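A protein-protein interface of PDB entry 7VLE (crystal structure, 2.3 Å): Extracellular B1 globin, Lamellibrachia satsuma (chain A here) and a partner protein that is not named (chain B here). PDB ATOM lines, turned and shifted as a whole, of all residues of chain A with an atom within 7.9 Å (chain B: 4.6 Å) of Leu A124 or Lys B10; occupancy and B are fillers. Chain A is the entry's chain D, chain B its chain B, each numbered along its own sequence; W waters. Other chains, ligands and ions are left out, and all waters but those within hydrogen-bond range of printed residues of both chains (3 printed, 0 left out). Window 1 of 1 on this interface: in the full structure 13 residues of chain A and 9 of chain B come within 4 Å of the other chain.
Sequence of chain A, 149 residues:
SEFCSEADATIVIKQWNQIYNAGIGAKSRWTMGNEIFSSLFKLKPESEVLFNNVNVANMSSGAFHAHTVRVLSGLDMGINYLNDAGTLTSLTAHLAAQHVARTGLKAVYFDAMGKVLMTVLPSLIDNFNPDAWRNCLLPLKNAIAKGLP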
ATOM      1  N   GLN A  15       5.202 -20.611  -6.693  1.00  0.00           N
ATOM      2  CA  GLN A  15       5.347 -21.463  -7.866  1.00  0.00           C
ATOM      3  C   GLN A  15       4.107 -21.443  -8.749  1.00  0.00           C
ATOM      4  O   GLN A  15       4.210 -21.711  -9.950  1.00  0.00           O
ATOM      5  CB  GLN A  15       5.669 -22.895  -7.437  1.00  0.00           C
ATOM      6  CG  GLN A  15       6.995 -23.035  -6.705  1.00  0.00           C
ATOM      7  CD  GLN A  15       7.400 -24.480  -6.484  1.00  0.00           C
ATOM      8  OE1 GLN A  15       6.553 -25.371  -6.405  1.00  0.00           O
ATOM      9  NE2 GLN A  15       8.702 -24.721  -6.391  1.00  0.00           N
ATOM     10  N   TRP A  16       2.941 -21.119  -8.183  1.00  0.00           N
ATOM     11  CA  TRP A  16       1.713 -21.047  -8.966  1.00  0.00           C
ATOM     12  C   TRP A  16       1.630 -19.761  -9.784  1.00  0.00           C
ATOM     13  O   TRP A  16       1.216 -19.794 -10.948  1.00  0.00           O
ATOM     14  CB  TRP A  16       0.500 -21.166  -8.044  1.00  0.00           C
ATOM     15  CG  TRP A  16      -0.802 -20.970  -8.748  1.00  0.00           C
ATOM     16  CD1 TRP A  16      -1.642 -19.901  -8.637  1.00  0.00           C
ATOM     17  CD2 TRP A  16      -1.412 -21.864  -9.686  1.00  0.00           C
ATOM     18  NE1 TRP A  16      -2.740 -20.077  -9.442  1.00  0.00           N
ATOM     19  CE2 TRP A  16      -2.624 -21.275 -10.096  1.00  0.00           C
ATOM     20  CE3 TRP A  16      -1.054 -23.109 -10.213  1.00  0.00           C
ATOM     21  CZ2 TRP A  16      -3.479 -21.886 -11.012  1.00  0.00           C
ATOM     22  CZ3 TRP A  16      -1.904 -23.714 -11.123  1.00  0.00           C
ATOM     23  CH2 TRP A  16      -3.102 -23.102 -11.512  1.00  0.00           C
ATOM     24  N   GLN A  18       3.958 -18.140 -10.919  1.00  0.00           N
ATOM     25  CA  GLN A  18       4.969 -18.333 -11.937  1.00  0.00           C
ATOM     26  C   GLN A  18       4.361 -18.763 -13.265  1.00  0.00           C
ATOM     27  O   GLN A  18       4.782 -18.303 -14.329  1.00  0.00           O
ATOM     28  CB  GLN A  18       5.920 -19.386 -11.394  1.00  0.00           C
ATOM     29  CG  GLN A  18       7.174 -19.593 -12.114  1.00  0.00           C
ATOM     30  CD  GLN A  18       7.941 -20.715 -11.480  1.00  0.00           C
ATOM     31  OE1 GLN A  18       7.907 -20.899 -10.261  1.00  0.00           O
ATOM     32  NE2 GLN A  18       8.613 -21.495 -12.298  1.00  0.00           N
ATOM     33  N   ILE A  19       3.373 -19.650 -13.224  1.00  0.00           N
ATOM     34  CA  ILE A  19       2.733 -20.156 -14.432  1.00  0.00           C
ATOM     35  C   ILE A  19       1.315 -19.651 -14.596  1.00  0.00           C
ATOM     36  O   ILE A  19       0.703 -19.898 -15.648  1.00  0.00           O
ATOM     37  CB  ILE A  19       2.740 -21.697 -14.464  1.00  0.00           C
ATOM     38  CG1 ILE A  19       1.917 -22.219 -13.291  1.00  0.00           C
ATOM     39  CG2 ILE A  19       4.166 -22.214 -14.393  1.00  0.00           C
ATOM     40  CD1 ILE A  19       1.585 -23.676 -13.375  1.00  0.00           C
ATOM     41  N   SER A  28      -2.629 -19.664 -23.001  1.00  0.00           N
ATOM     42  CA  SER A  28      -1.860 -20.547 -22.134  1.00  0.00           C
ATOM     43  C   SER A  28      -2.715 -21.079 -20.995  1.00  0.00           C
ATOM     44  O   SER A  28      -2.423 -22.149 -20.448  1.00  0.00           O
ATOM     45  CB  SER A  28      -0.658 -19.801 -21.578  1.00  0.00           C
ATOM     46  OG  SER A  28      -1.128 -18.747 -20.779  1.00  0.00           O
ATOM     47  N   THR A  31      -4.590 -23.984 -22.595  1.00  0.00           N
ATOM     48  CA  THR A  31      -3.595 -24.993 -22.945  1.00  0.00           C
ATOM     49  C   THR A  31      -3.289 -25.876 -21.745  1.00  0.00           C
ATOM     50  O   THR A  31      -3.309 -27.109 -21.839  1.00  0.00           O
ATOM     51  CB  THR A  31      -2.311 -24.331 -23.446  1.00  0.00           C
ATOM     52  OG1 THR A  31      -2.589 -23.546 -24.611  1.00  0.00           O
ATOM     53  CG2 THR A  31      -1.269 -25.389 -23.783  1.00  0.00           C
ATOM     54  N   MET A  32      -2.987 -25.251 -20.605  1.00  0.00           N
ATOM     55  CA  MET A  32      -2.831 -25.996 -19.364  1.00  0.00           C
ATOM     56  C   MET A  32      -4.113 -26.733 -19.006  1.00  0.00           C
ATOM     57  O   MET A  32      -4.075 -27.900 -18.602  1.00  0.00           O
ATOM     58  CB  MET A  32      -2.430 -25.048 -18.233  1.00  0.00           C
ATOM     59  CG  MET A  32      -1.046 -24.442 -18.380  1.00  0.00           C
ATOM     60  SD  MET A  32      -0.717 -23.215 -17.101  1.00  0.00           S
ATOM     61  CE  MET A  32      -1.259 -24.099 -15.642  1.00  0.00           C
ATOM     62  N   GLY A  33      -5.260 -26.067 -19.156  1.00  0.00           N
ATOM     63  CA  GLY A  33      -6.525 -26.709 -18.843  1.00  0.00           C
ATOM     64  C   GLY A  33      -6.811 -27.904 -19.731  1.00  0.00           C
ATOM     65  O   GLY A  33      -7.298 -28.935 -19.261  1.00  0.00           O
ATOM     66  N   GLU A  35      -4.534 -29.788 -21.279  1.00  0.00           N
ATOM     67  CA  GLU A  35      -3.610 -30.849 -20.884  1.00  0.00           C
ATOM     68  C   GLU A  35      -4.071 -31.535 -19.605  1.00  0.00           C
ATOM     69  O   GLU A  35      -3.983 -32.762 -19.481  1.00  0.00           O
ATOM     70  CB  GLU A  35      -2.203 -30.278 -20.705  1.00  0.00           C
ATOM     71  CG  GLU A  35      -1.548 -29.822 -21.995  1.00  0.00           C
ATOM     72  CD  GLU A  35      -1.329 -30.965 -22.965  1.00  0.00           C
ATOM     73  OE1 GLU A  35      -0.711 -31.974 -22.566  1.00  0.00           O
ATOM     74  OE2 GLU A  35      -1.787 -30.859 -24.121  1.00  0.00           O
ATOM     75  N   ILE A  36      -4.572 -30.755 -18.645  1.00  0.00           N
ATOM     76  CA  ILE A  36      -4.999 -31.308 -17.361  1.00  0.00           C
ATOM     77  C   ILE A  36      -6.197 -32.230 -17.545  1.00  0.00           C
ATOM     78  O   ILE A  36      -6.234 -33.343 -17.006  1.00  0.00           O
ATOM     79  CB  ILE A  36      -5.319 -30.174 -16.370  1.00  0.00           C
ATOM     80  CG1 ILE A  36      -4.045 -29.459 -15.924  1.00  0.00           C
ATOM     81  CG2 ILE A  36      -6.071 -30.714 -15.165  1.00  0.00           C
ATOM     82  CD1 ILE A  36      -4.306 -28.325 -14.957  1.00  0.00           C
ATOM     83  N   LEU A 117      -2.482 -33.202 -11.553  1.00  0.00           N
ATOM     84  CA  LEU A 117      -1.804 -31.969 -11.174  1.00  0.00           C
ATOM     85  C   LEU A 117      -0.370 -32.242 -10.741  1.00  0.00           C
ATOM     86  O   LEU A 117       0.556 -31.534 -11.154  1.00  0.00           O
ATOM     87  CB  LEU A 117      -2.583 -31.268 -10.060  1.00  0.00           C
ATOM     88  CG  LEU A 117      -3.974 -30.756 -10.446  1.00  0.00           C
ATOM     89  CD1 LEU A 117      -4.696 -30.161  -9.246  1.00  0.00           C
ATOM     90  CD2 LEU A 117      -3.865 -29.734 -11.561  1.00  0.00           C
ATOM     91  N   THR A 119       1.415 -34.505 -11.791  1.00  0.00           N
ATOM     92  CA  THR A 119       2.138 -34.943 -12.979  1.00  0.00           C
ATOM     93  C   THR A 119       2.442 -33.788 -13.929  1.00  0.00           C
ATOM     94  O   THR A 119       3.565 -33.683 -14.435  1.00  0.00           O
ATOM     95  CB  THR A 119       1.333 -36.021 -13.715  1.00  0.00           C
ATOM     96  OG1 THR A 119       1.249 -37.199 -12.902  1.00  0.00           O
ATOM     97  CG2 THR A 119       1.986 -36.371 -15.044  1.00  0.00           C
ATOM     98  N   VAL A 120       1.463 -32.912 -14.166  1.00  0.00           N
ATOM     99  CA  VAL A 120       1.605 -31.858 -15.168  1.00  0.00           C
ATOM    100  C   VAL A 120       2.474 -30.720 -14.652  1.00  0.00           C
ATOM    101  O   VAL A 120       3.400 -30.269 -15.337  1.00  0.00           O
ATOM    102  CB  VAL A 120       0.219 -31.340 -15.594  1.00  0.00           C
ATOM    103  CG1 VAL A 120       0.367 -30.118 -16.490  1.00  0.00           C
ATOM    104  CG2 VAL A 120      -0.577 -32.430 -16.292  1.00  0.00           C
ATOM    105  N   LEU A 121       2.173 -30.227 -13.453  1.00  0.00           N
ATOM    106  CA  LEU A 121       2.812 -29.017 -12.936  1.00  0.00           C
ATOM    107  C   LEU A 121       4.337 -29.050 -12.929  1.00  0.00           C
ATOM    108  O   LEU A 121       4.943 -28.001 -13.211  1.00  0.00           O
ATOM    109  CB  LEU A 121       2.284 -28.728 -11.524  1.00  0.00           C
ATOM    110  CG  LEU A 121       0.809 -28.340 -11.458  1.00  0.00           C
ATOM    111  CD1 LEU A 121       0.391 -28.064 -10.025  1.00  0.00           C
ATOM    112  CD2 LEU A 121       0.541 -27.136 -12.345  1.00  0.00           C
ATOM    113  N   PRO A 122       5.015 -30.157 -12.603  1.00  0.00           N
ATOM    114  CA  PRO A 122       6.485 -30.153 -12.708  1.00  0.00           C
ATOM    115  C   PRO A 122       6.993 -29.856 -14.107  1.00  0.00           C
ATOM    116  O   PRO A 122       8.082 -29.285 -14.250  1.00  0.00           O
ATOM    117  CB  PRO A 122       6.876 -31.567 -12.249  1.00  0.00           C
ATOM    118  CG  PRO A 122       5.610 -32.367 -12.290  1.00  0.00           C
ATOM    119  CD  PRO A 122       4.529 -31.396 -11.971  1.00  0.00           C
ATOM    120  N   SER A 123       6.240 -30.226 -15.147  1.00  0.00           N
ATOM    121  CA  SER A 123       6.633 -29.889 -16.510  1.00  0.00           C
ATOM    122  C   SER A 123       6.575 -28.391 -16.767  1.00  0.00           C
ATOM    123  O   SER A 123       7.210 -27.909 -17.710  1.00  0.00           O
ATOM    124  CB  SER A 123       5.737 -30.611 -17.516  1.00  0.00           C
ATOM    125  OG  SER A 123       5.619 -31.988 -17.208  1.00  0.00           O
ATOM    126  N   LEU A 124       5.827 -27.652 -15.948  1.00  0.00           N
ATOM    127  CA  LEU A 124       5.622 -26.224 -16.129  1.00  0.00           C
ATOM    128  C   LEU A 124       6.391 -25.359 -15.143  1.00  0.00           C
ATOM    129  O   LEU A 124       6.729 -24.223 -15.479  1.00  0.00           O
ATOM    130  CB  LEU A 124       4.129 -25.889 -16.009  1.00  0.00           C
ATOM    131  CG  LEU A 124       3.195 -26.366 -17.123  1.00  0.00           C
ATOM    132  CD1 LEU A 124       1.744 -26.244 -16.689  1.00  0.00           C
ATOM    133  CD2 LEU A 124       3.439 -25.563 -18.388  1.00  0.00           C
ATOM    134  N   ILE A 125       6.690 -25.867 -13.950  1.00  0.00           N
ATOM    135  CA  ILE A 125       7.138 -25.048 -12.828  1.00  0.00           C
ATOM    136  C   ILE A 125       8.617 -25.298 -12.560  1.00  0.00           C
ATOM    137  O   ILE A 125       9.064 -26.450 -12.510  1.00  0.00           O
ATOM    138  CB  ILE A 125       6.296 -25.328 -11.571  1.00  0.00           C
ATOM    139  CG1 ILE A 125       4.876 -24.790 -11.762  1.00  0.00           C
ATOM    140  CG2 ILE A 125       6.945 -24.720 -10.338  1.00  0.00           C
ATOM    141  CD1 ILE A 125       3.947 -25.088 -10.609  1.00  0.00           C
ATOM    142  N   ASP A 126       9.370 -24.212 -12.381  1.00  0.00           N
ATOM    143  CA  ASP A 126      10.767 -24.299 -11.973  1.00  0.00           C
ATOM    144  C   ASP A 126      10.871 -24.805 -10.539  1.00  0.00           C
ATOM    145  O   ASP A 126      10.215 -24.274  -9.636  1.00  0.00           O
ATOM    146  CB  ASP A 126      11.442 -22.932 -12.086  1.00  0.00           C
ATOM    147  CG  ASP A 126      11.681 -22.512 -13.520  1.00  0.00           C
ATOM    148  OD1 ASP A 126      11.495 -23.349 -14.425  1.00  0.00           O
ATOM    149  OD2 ASP A 126      12.058 -21.341 -13.740  1.00  0.00           O
ATOM    150  N   ASN A 127      11.707 -25.821 -10.333  1.00  0.00           N
ATOM    151  CA  ASN A 127      11.960 -26.391  -9.008  1.00  0.00           C
ATOM    152  C   ASN A 127      10.661 -26.764  -8.298  1.00  0.00           C
ATOM    153  O   ASN A 127      10.455 -26.436  -7.126  1.00  0.00           O
ATOM    154  CB  ASN A 127      12.781 -25.434  -8.143  1.00  0.00           C
ATOM    155  CG  ASN A 127      14.268 -25.642  -8.289  1.00  0.00           C
ATOM    156  OD1 ASN A 127      15.019 -24.688  -8.476  1.00  0.00           O
ATOM    157  ND2 ASN A 127      14.705 -26.893  -8.201  1.00  0.00           N
ATOM    158  N   PHE A 128       9.776 -27.447  -9.022  1.00  0.00           N
ATOM    159  CA  PHE A 128       8.505 -27.872  -8.448  1.00  0.00           C
ATOM    160  C   PHE A 128       8.735 -28.660  -7.165  1.00  0.00           C
ATOM    161  O   PHE A 128       9.522 -29.609  -7.137  1.00  0.00           O
ATOM    162  CB  PHE A 128       7.729 -28.720  -9.460  1.00  0.00           C
ATOM    163  CG  PHE A 128       6.415 -29.241  -8.939  1.00  0.00           C
ATOM    164  CD1 PHE A 128       5.293 -28.428  -8.916  1.00  0.00           C
ATOM    165  CD2 PHE A 128       6.302 -30.544  -8.482  1.00  0.00           C
ATOM    166  CE1 PHE A 128       4.084 -28.905  -8.439  1.00  0.00           C
ATOM    167  CE2 PHE A 128       5.095 -31.026  -8.006  1.00  0.00           C
ATOM    168  CZ  PHE A 128       3.986 -30.205  -7.984  1.00  0.00           C
ATOM    169  N   LEU B   6       3.138 -28.320 -23.076  1.00  0.00           N
ATOM    170  CA  LEU B   6       3.714 -27.960 -21.786  1.00  0.00           C
ATOM    171  C   LEU B   6       5.165 -27.520 -21.929  1.00  0.00           C
ATOM    172  O   LEU B   6       5.579 -26.521 -21.329  1.00  0.00           O
ATOM    173  CB  LEU B   6       3.610 -29.142 -20.824  1.00  0.00           C
ATOM    174  CG  LEU B   6       2.202 -29.631 -20.485  1.00  0.00           C
ATOM    175  CD1 LEU B   6       2.266 -30.893 -19.641  1.00  0.00           C
ATOM    176  CD2 LEU B   6       1.429 -28.540 -19.766  1.00  0.00           C
ATOM    177  N   GLN B   7       5.953 -28.261 -22.713  1.00  0.00           N
ATOM    178  CA  GLN B   7       7.357 -27.913 -22.907  1.00  0.00           C
ATOM    179  C   GLN B   7       7.501 -26.565 -23.598  1.00  0.00           C
ATOM    180  O   GLN B   7       8.430 -25.803 -23.304  1.00  0.00           O
ATOM    181  CB  GLN B   7       8.066 -28.997 -23.719  1.00  0.00           C
ATOM    182  CG  GLN B   7       8.328 -30.288 -22.963  1.00  0.00           C
ATOM    183  CD  GLN B   7       7.080 -31.127 -22.783  1.00  0.00           C
ATOM    184  OE1 GLN B   7       6.181 -31.116 -23.623  1.00  0.00           O
ATOM    185  NE2 GLN B   7       7.017 -31.859 -21.677  1.00  0.00           N
ATOM    186  N   ARG B   8       6.596 -26.260 -24.530  1.00  0.00           N
ATOM    187  CA  ARG B   8       6.636 -24.968 -25.205  1.00  0.00           C
ATOM    188  C   ARG B   8       6.388 -23.830 -24.224  1.00  0.00           C
ATOM    189  O   ARG B   8       7.011 -22.768 -24.323  1.00  0.00           O
ATOM    190  CB  ARG B   8       5.613 -24.947 -26.342  1.00  0.00           C
ATOM    191  CG  ARG B   8       5.992 -25.854 -27.500  1.00  0.00           C
ATOM    192  CD  ARG B   8       4.796 -26.266 -28.343  1.00  0.00           C
ATOM    193  NE  ARG B   8       5.164 -27.319 -29.286  1.00  0.00           N
ATOM    194  CZ  ARG B   8       5.484 -27.110 -30.558  1.00  0.00           C
ATOM    195  NH1 ARG B   8       5.469 -25.882 -31.057  1.00  0.00           N
ATOM    196  NH2 ARG B   8       5.813 -28.133 -31.336  1.00  0.00           N
ATOM    197  N   LEU B   9       5.491 -24.044 -23.259  1.00  0.00           N
ATOM    198  CA  LEU B   9       5.228 -23.035 -22.239  1.00  0.00           C
ATOM    199  C   LEU B   9       6.446 -22.822 -21.347  1.00  0.00           C
ATOM    200  O   LEU B   9       6.827 -21.681 -21.061  1.00  0.00           O
ATOM    201  CB  LEU B   9       4.014 -23.441 -21.403  1.00  0.00           C
ATOM    202  CG  LEU B   9       2.652 -23.368 -22.092  1.00  0.00           C
ATOM    203  CD1 LEU B   9       1.549 -23.799 -21.139  1.00  0.00           C
ATOM    204  CD2 LEU B   9       2.402 -21.960 -22.606  1.00  0.00           C
ATOM    205  N   LYS B  10       7.063 -23.915 -20.889  1.00  0.00           N
ATOM    206  CA  LYS B  10       8.246 -23.812 -20.037  1.00  0.00           C
ATOM    207  C   LYS B  10       9.383 -23.097 -20.758  1.00  0.00           C
ATOM    208  O   LYS B  10       9.999 -22.174 -20.211  1.00  0.00           O
ATOM    209  CB  LYS B  10       8.685 -25.208 -19.589  1.00  0.00           C
ATOM    210  CG  LYS B  10       9.995 -25.231 -18.816  1.00  0.00           C
ATOM    211  CD  LYS B  10       9.778 -25.185 -17.310  1.00  0.00           C
ATOM    212  CE  LYS B  10       9.920 -26.569 -16.692  1.00  0.00           C
ATOM    213  NZ  LYS B  10      10.115 -26.528 -15.217  1.00  0.00           N
ATOM    214  N   VAL B  11       9.677 -23.519 -21.993  1.00  0.00           N
ATOM    215  CA  VAL B  11      10.732 -22.887 -22.784  1.00  0.00           C
ATOM    216  C   VAL B  11      10.450 -21.401 -22.967  1.00  0.00           C
ATOM    217  O   VAL B  11      11.363 -20.567 -22.901  1.00  0.00           O
ATOM    218  CB  VAL B  11      10.878 -23.601 -24.142  1.00  0.00           C
ATOM    219  CG1 VAL B  11      11.722 -22.773 -25.097  1.00  0.00           C
ATOM    220  CG2 VAL B  11      11.482 -24.985 -23.959  1.00  0.00           C
ATOM    221  N   LYS B  12       9.184 -21.050 -23.206  1.00  0.00           N
ATOM    222  CA  LYS B  12       8.805 -19.650 -23.379  1.00  0.00           C
ATOM    223  C   LYS B  12       9.216 -18.813 -22.175  1.00  0.00           C
ATOM    224  O   LYS B  12       9.882 -17.780 -22.317  1.00  0.00           O
ATOM    225  CB  LYS B  12       7.296 -19.544 -23.602  1.00  0.00           C
ATOM    226  CG  LYS B  12       6.849 -19.684 -25.043  1.00  0.00           C
ATOM    227  CD  LYS B  12       5.339 -19.828 -25.119  1.00  0.00           C
ATOM    228  CE  LYS B  12       4.840 -19.708 -26.545  1.00  0.00           C
ATOM    229  NZ  LYS B  12       4.956 -18.315 -27.057  1.00  0.00           N
ATOM    230  N   ARG B  13       8.821 -19.247 -20.976  1.00  0.00           N
ATOM    231  CA  ARG B  13       9.109 -18.479 -19.770  1.00  0.00           C
ATOM    232  C   ARG B  13      10.599 -18.477 -19.454  1.00  0.00           C
ATOM    233  O   ARG B  13      11.148 -17.448 -19.041  1.00  0.00           O
ATOM    234  CB  ARG B  13       8.308 -19.044 -18.598  1.00  0.00           C
ATOM    235  CG  ARG B  13       8.531 -18.328 -17.281  1.00  0.00           C
ATOM    236  CD  ARG B  13       7.716 -18.968 -16.172  1.00  0.00           C
ATOM    237  NE  ARG B  13       7.935 -20.410 -16.099  1.00  0.00           N
ATOM    238  CZ  ARG B  13       8.897 -20.985 -15.386  1.00  0.00           C
ATOM    239  NH1 ARG B  13       9.023 -22.306 -15.378  1.00  0.00           N
ATOM    240  NH2 ARG B  13       9.737 -20.238 -14.680  1.00  0.00           N
ATOM    241  N   GLN B  14      11.270 -19.615 -19.640  1.00  0.00           N
ATOM    242  CA  GLN B  14      12.702 -19.679 -19.367  1.00  0.00           C
ATOM    243  C   GLN B  14      13.490 -18.814 -20.345  1.00  0.00           C
ATOM    244  O   GLN B  14      14.501 -18.208 -19.968  1.00  0.00           O
ATOM    245  CB  GLN B  14      13.189 -21.129 -19.412  1.00  0.00           C
ATOM    246  CG  GLN B  14      12.757 -21.967 -18.215  1.00  0.00           C
ATOM    247  CD  GLN B  14      13.604 -23.216 -18.032  1.00  0.00           C
ATOM    248  OE1 GLN B  14      14.318 -23.637 -18.942  1.00  0.00           O
ATOM    249  NE2 GLN B  14      13.532 -23.811 -16.846  1.00  0.00           N
ATOM    250  N   ASP B 126      15.589 -26.703 -17.875  1.00  0.00           N
ATOM    251  CA  ASP B 126      14.869 -27.887 -18.349  1.00  0.00           C
ATOM    252  C   ASP B 126      15.506 -28.336 -19.663  1.00  0.00           C
ATOM    253  O   ASP B 126      15.123 -27.890 -20.745  1.00  0.00           O
ATOM    254  CB  ASP B 126      13.385 -27.576 -18.522  1.00  0.00           C
ATOM    255  CG  ASP B 126      12.537 -28.823 -18.722  1.00  0.00           C
ATOM    256  OD1 ASP B 126      11.362 -28.815 -18.299  1.00  0.00           O
ATOM    257  OD2 ASP B 126      13.038 -29.815 -19.291  1.00  0.00           O
HETATM  258  O   HOH W   1       8.923 -29.203 -19.604  1.00  0.00           O
HETATM  259  O   HOH W   2       6.065 -22.497 -17.523  1.00  0.00           O
HETATM  260  O   HOH W   3      12.480 -26.600 -14.162  1.00  0.00           O
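The backbone carbonyl oxygen of Leu A124 lies within hydrogen-bond range of the guanidinium group of Arg B13, 3.0 Å away.
The side-chain amino group (NZ) of Lys B10 lies within hydrogen-bond range of the backbone carbonyl oxygen (O) of Ile A125 (2.9 Å).
The guanidinium group (NH2) of Arg B13 lies close to the side-chain amide nitrogen (NE2) of Gln A18.
The guanidinium group (NH2) of Arg B13 lies within salt-bridge range of the side-chain carboxylate (OD2) of Asp A126 (2.7 Å).
OD1 of Asp A126 is in salt-bridge range of NZ of Lys B10 (3.6 Å).
The side-chain amide nitrogen (NE2) of Gln B14 is in hydrogen-bond range of the side-chain carboxylate (OD1) of Asp A126.
The side-chain amide nitrogen (NE2) of Gln A18 lies close to the backbone NH (N) of Asp A126, at 2.8 Å.
OE1 of Gln B14 sits at hydrogen-bond distance from N of Asp B126 (3.5 Å).
OG of Ser A123 lies close to O of Val A120 (3.4 Å).
Among the printed residues, merely in contact across the chains: Ser A123 with Lys B10 (3.2 Å), Pro A122 with Lys B10 (3.6 Å), Leu A124 with Lys B10 (3.7 Å), Leu A124 with Leu B9 (3.7 Å), Val A120 with Leu B6 (3.8 Å), Leu A124 with Leu B6 (3.8 Å), Met A32 with Leu B9 (3.8 Å), Ser A28 with Leu B9 (3.9 Å) and Glu A35 with Leu B6 (3.9 Å).
Leu A124 touches just these residues of chain B: Leu B6 (3.8 Å), Leu B9 (3.7 Å), Lys B10 (3.7 Å) and Arg B13 (3.0 Å).
Printed residues of chain A within 4 Å of Lys B10: Pro A122, Ser A123, Leu A124, Ile A125 and Asp A126.
Of the printed residues of chain A, Arg B13 touches Gln A18 (2.9 Å), Leu A124 (3.0 Å) and Asp A126 (2.7 Å).
Of the printed residues of chain B, Glu A35 touches Leu B6 (3.9 Å).
Of the printed residues of chain A, Gln B14 touches Asp A126.
Printed residues of chain B within 4 Å of Ser A28: Leu B9.
Gly A33 touches none of the printed residues of chain B.
The nearest residue of chain A that does not touch Lys B10 is Asn A127 (5.2 Å).
Of the 21 printed residues of chain A, 10 touch a printed residue of chain B.
Printed residues of chain A that touch a printed residue of chain B: Gln A18, Ser A28, Met A32, Glu A35, Val A120, Pro A122, Ser A123, Leu A124, Ile A125 and Asp A126.
Among the printed residues, 15 pairs touch across the chains.
Water W3 bridges NZ of Lys B10 (2.6 Å) and OD1 of Asp A126 (3.4 Å).
Water W2 lies within hydrogen-bond range of the backbone carbonyl oxygen of Leu A124 (2.8 Å) and the guanidinium group of Arg B13 (3.1 Å).
Water W1 lies within hydrogen-bond range of OD1 of Asp B126 and O of Ser A123.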
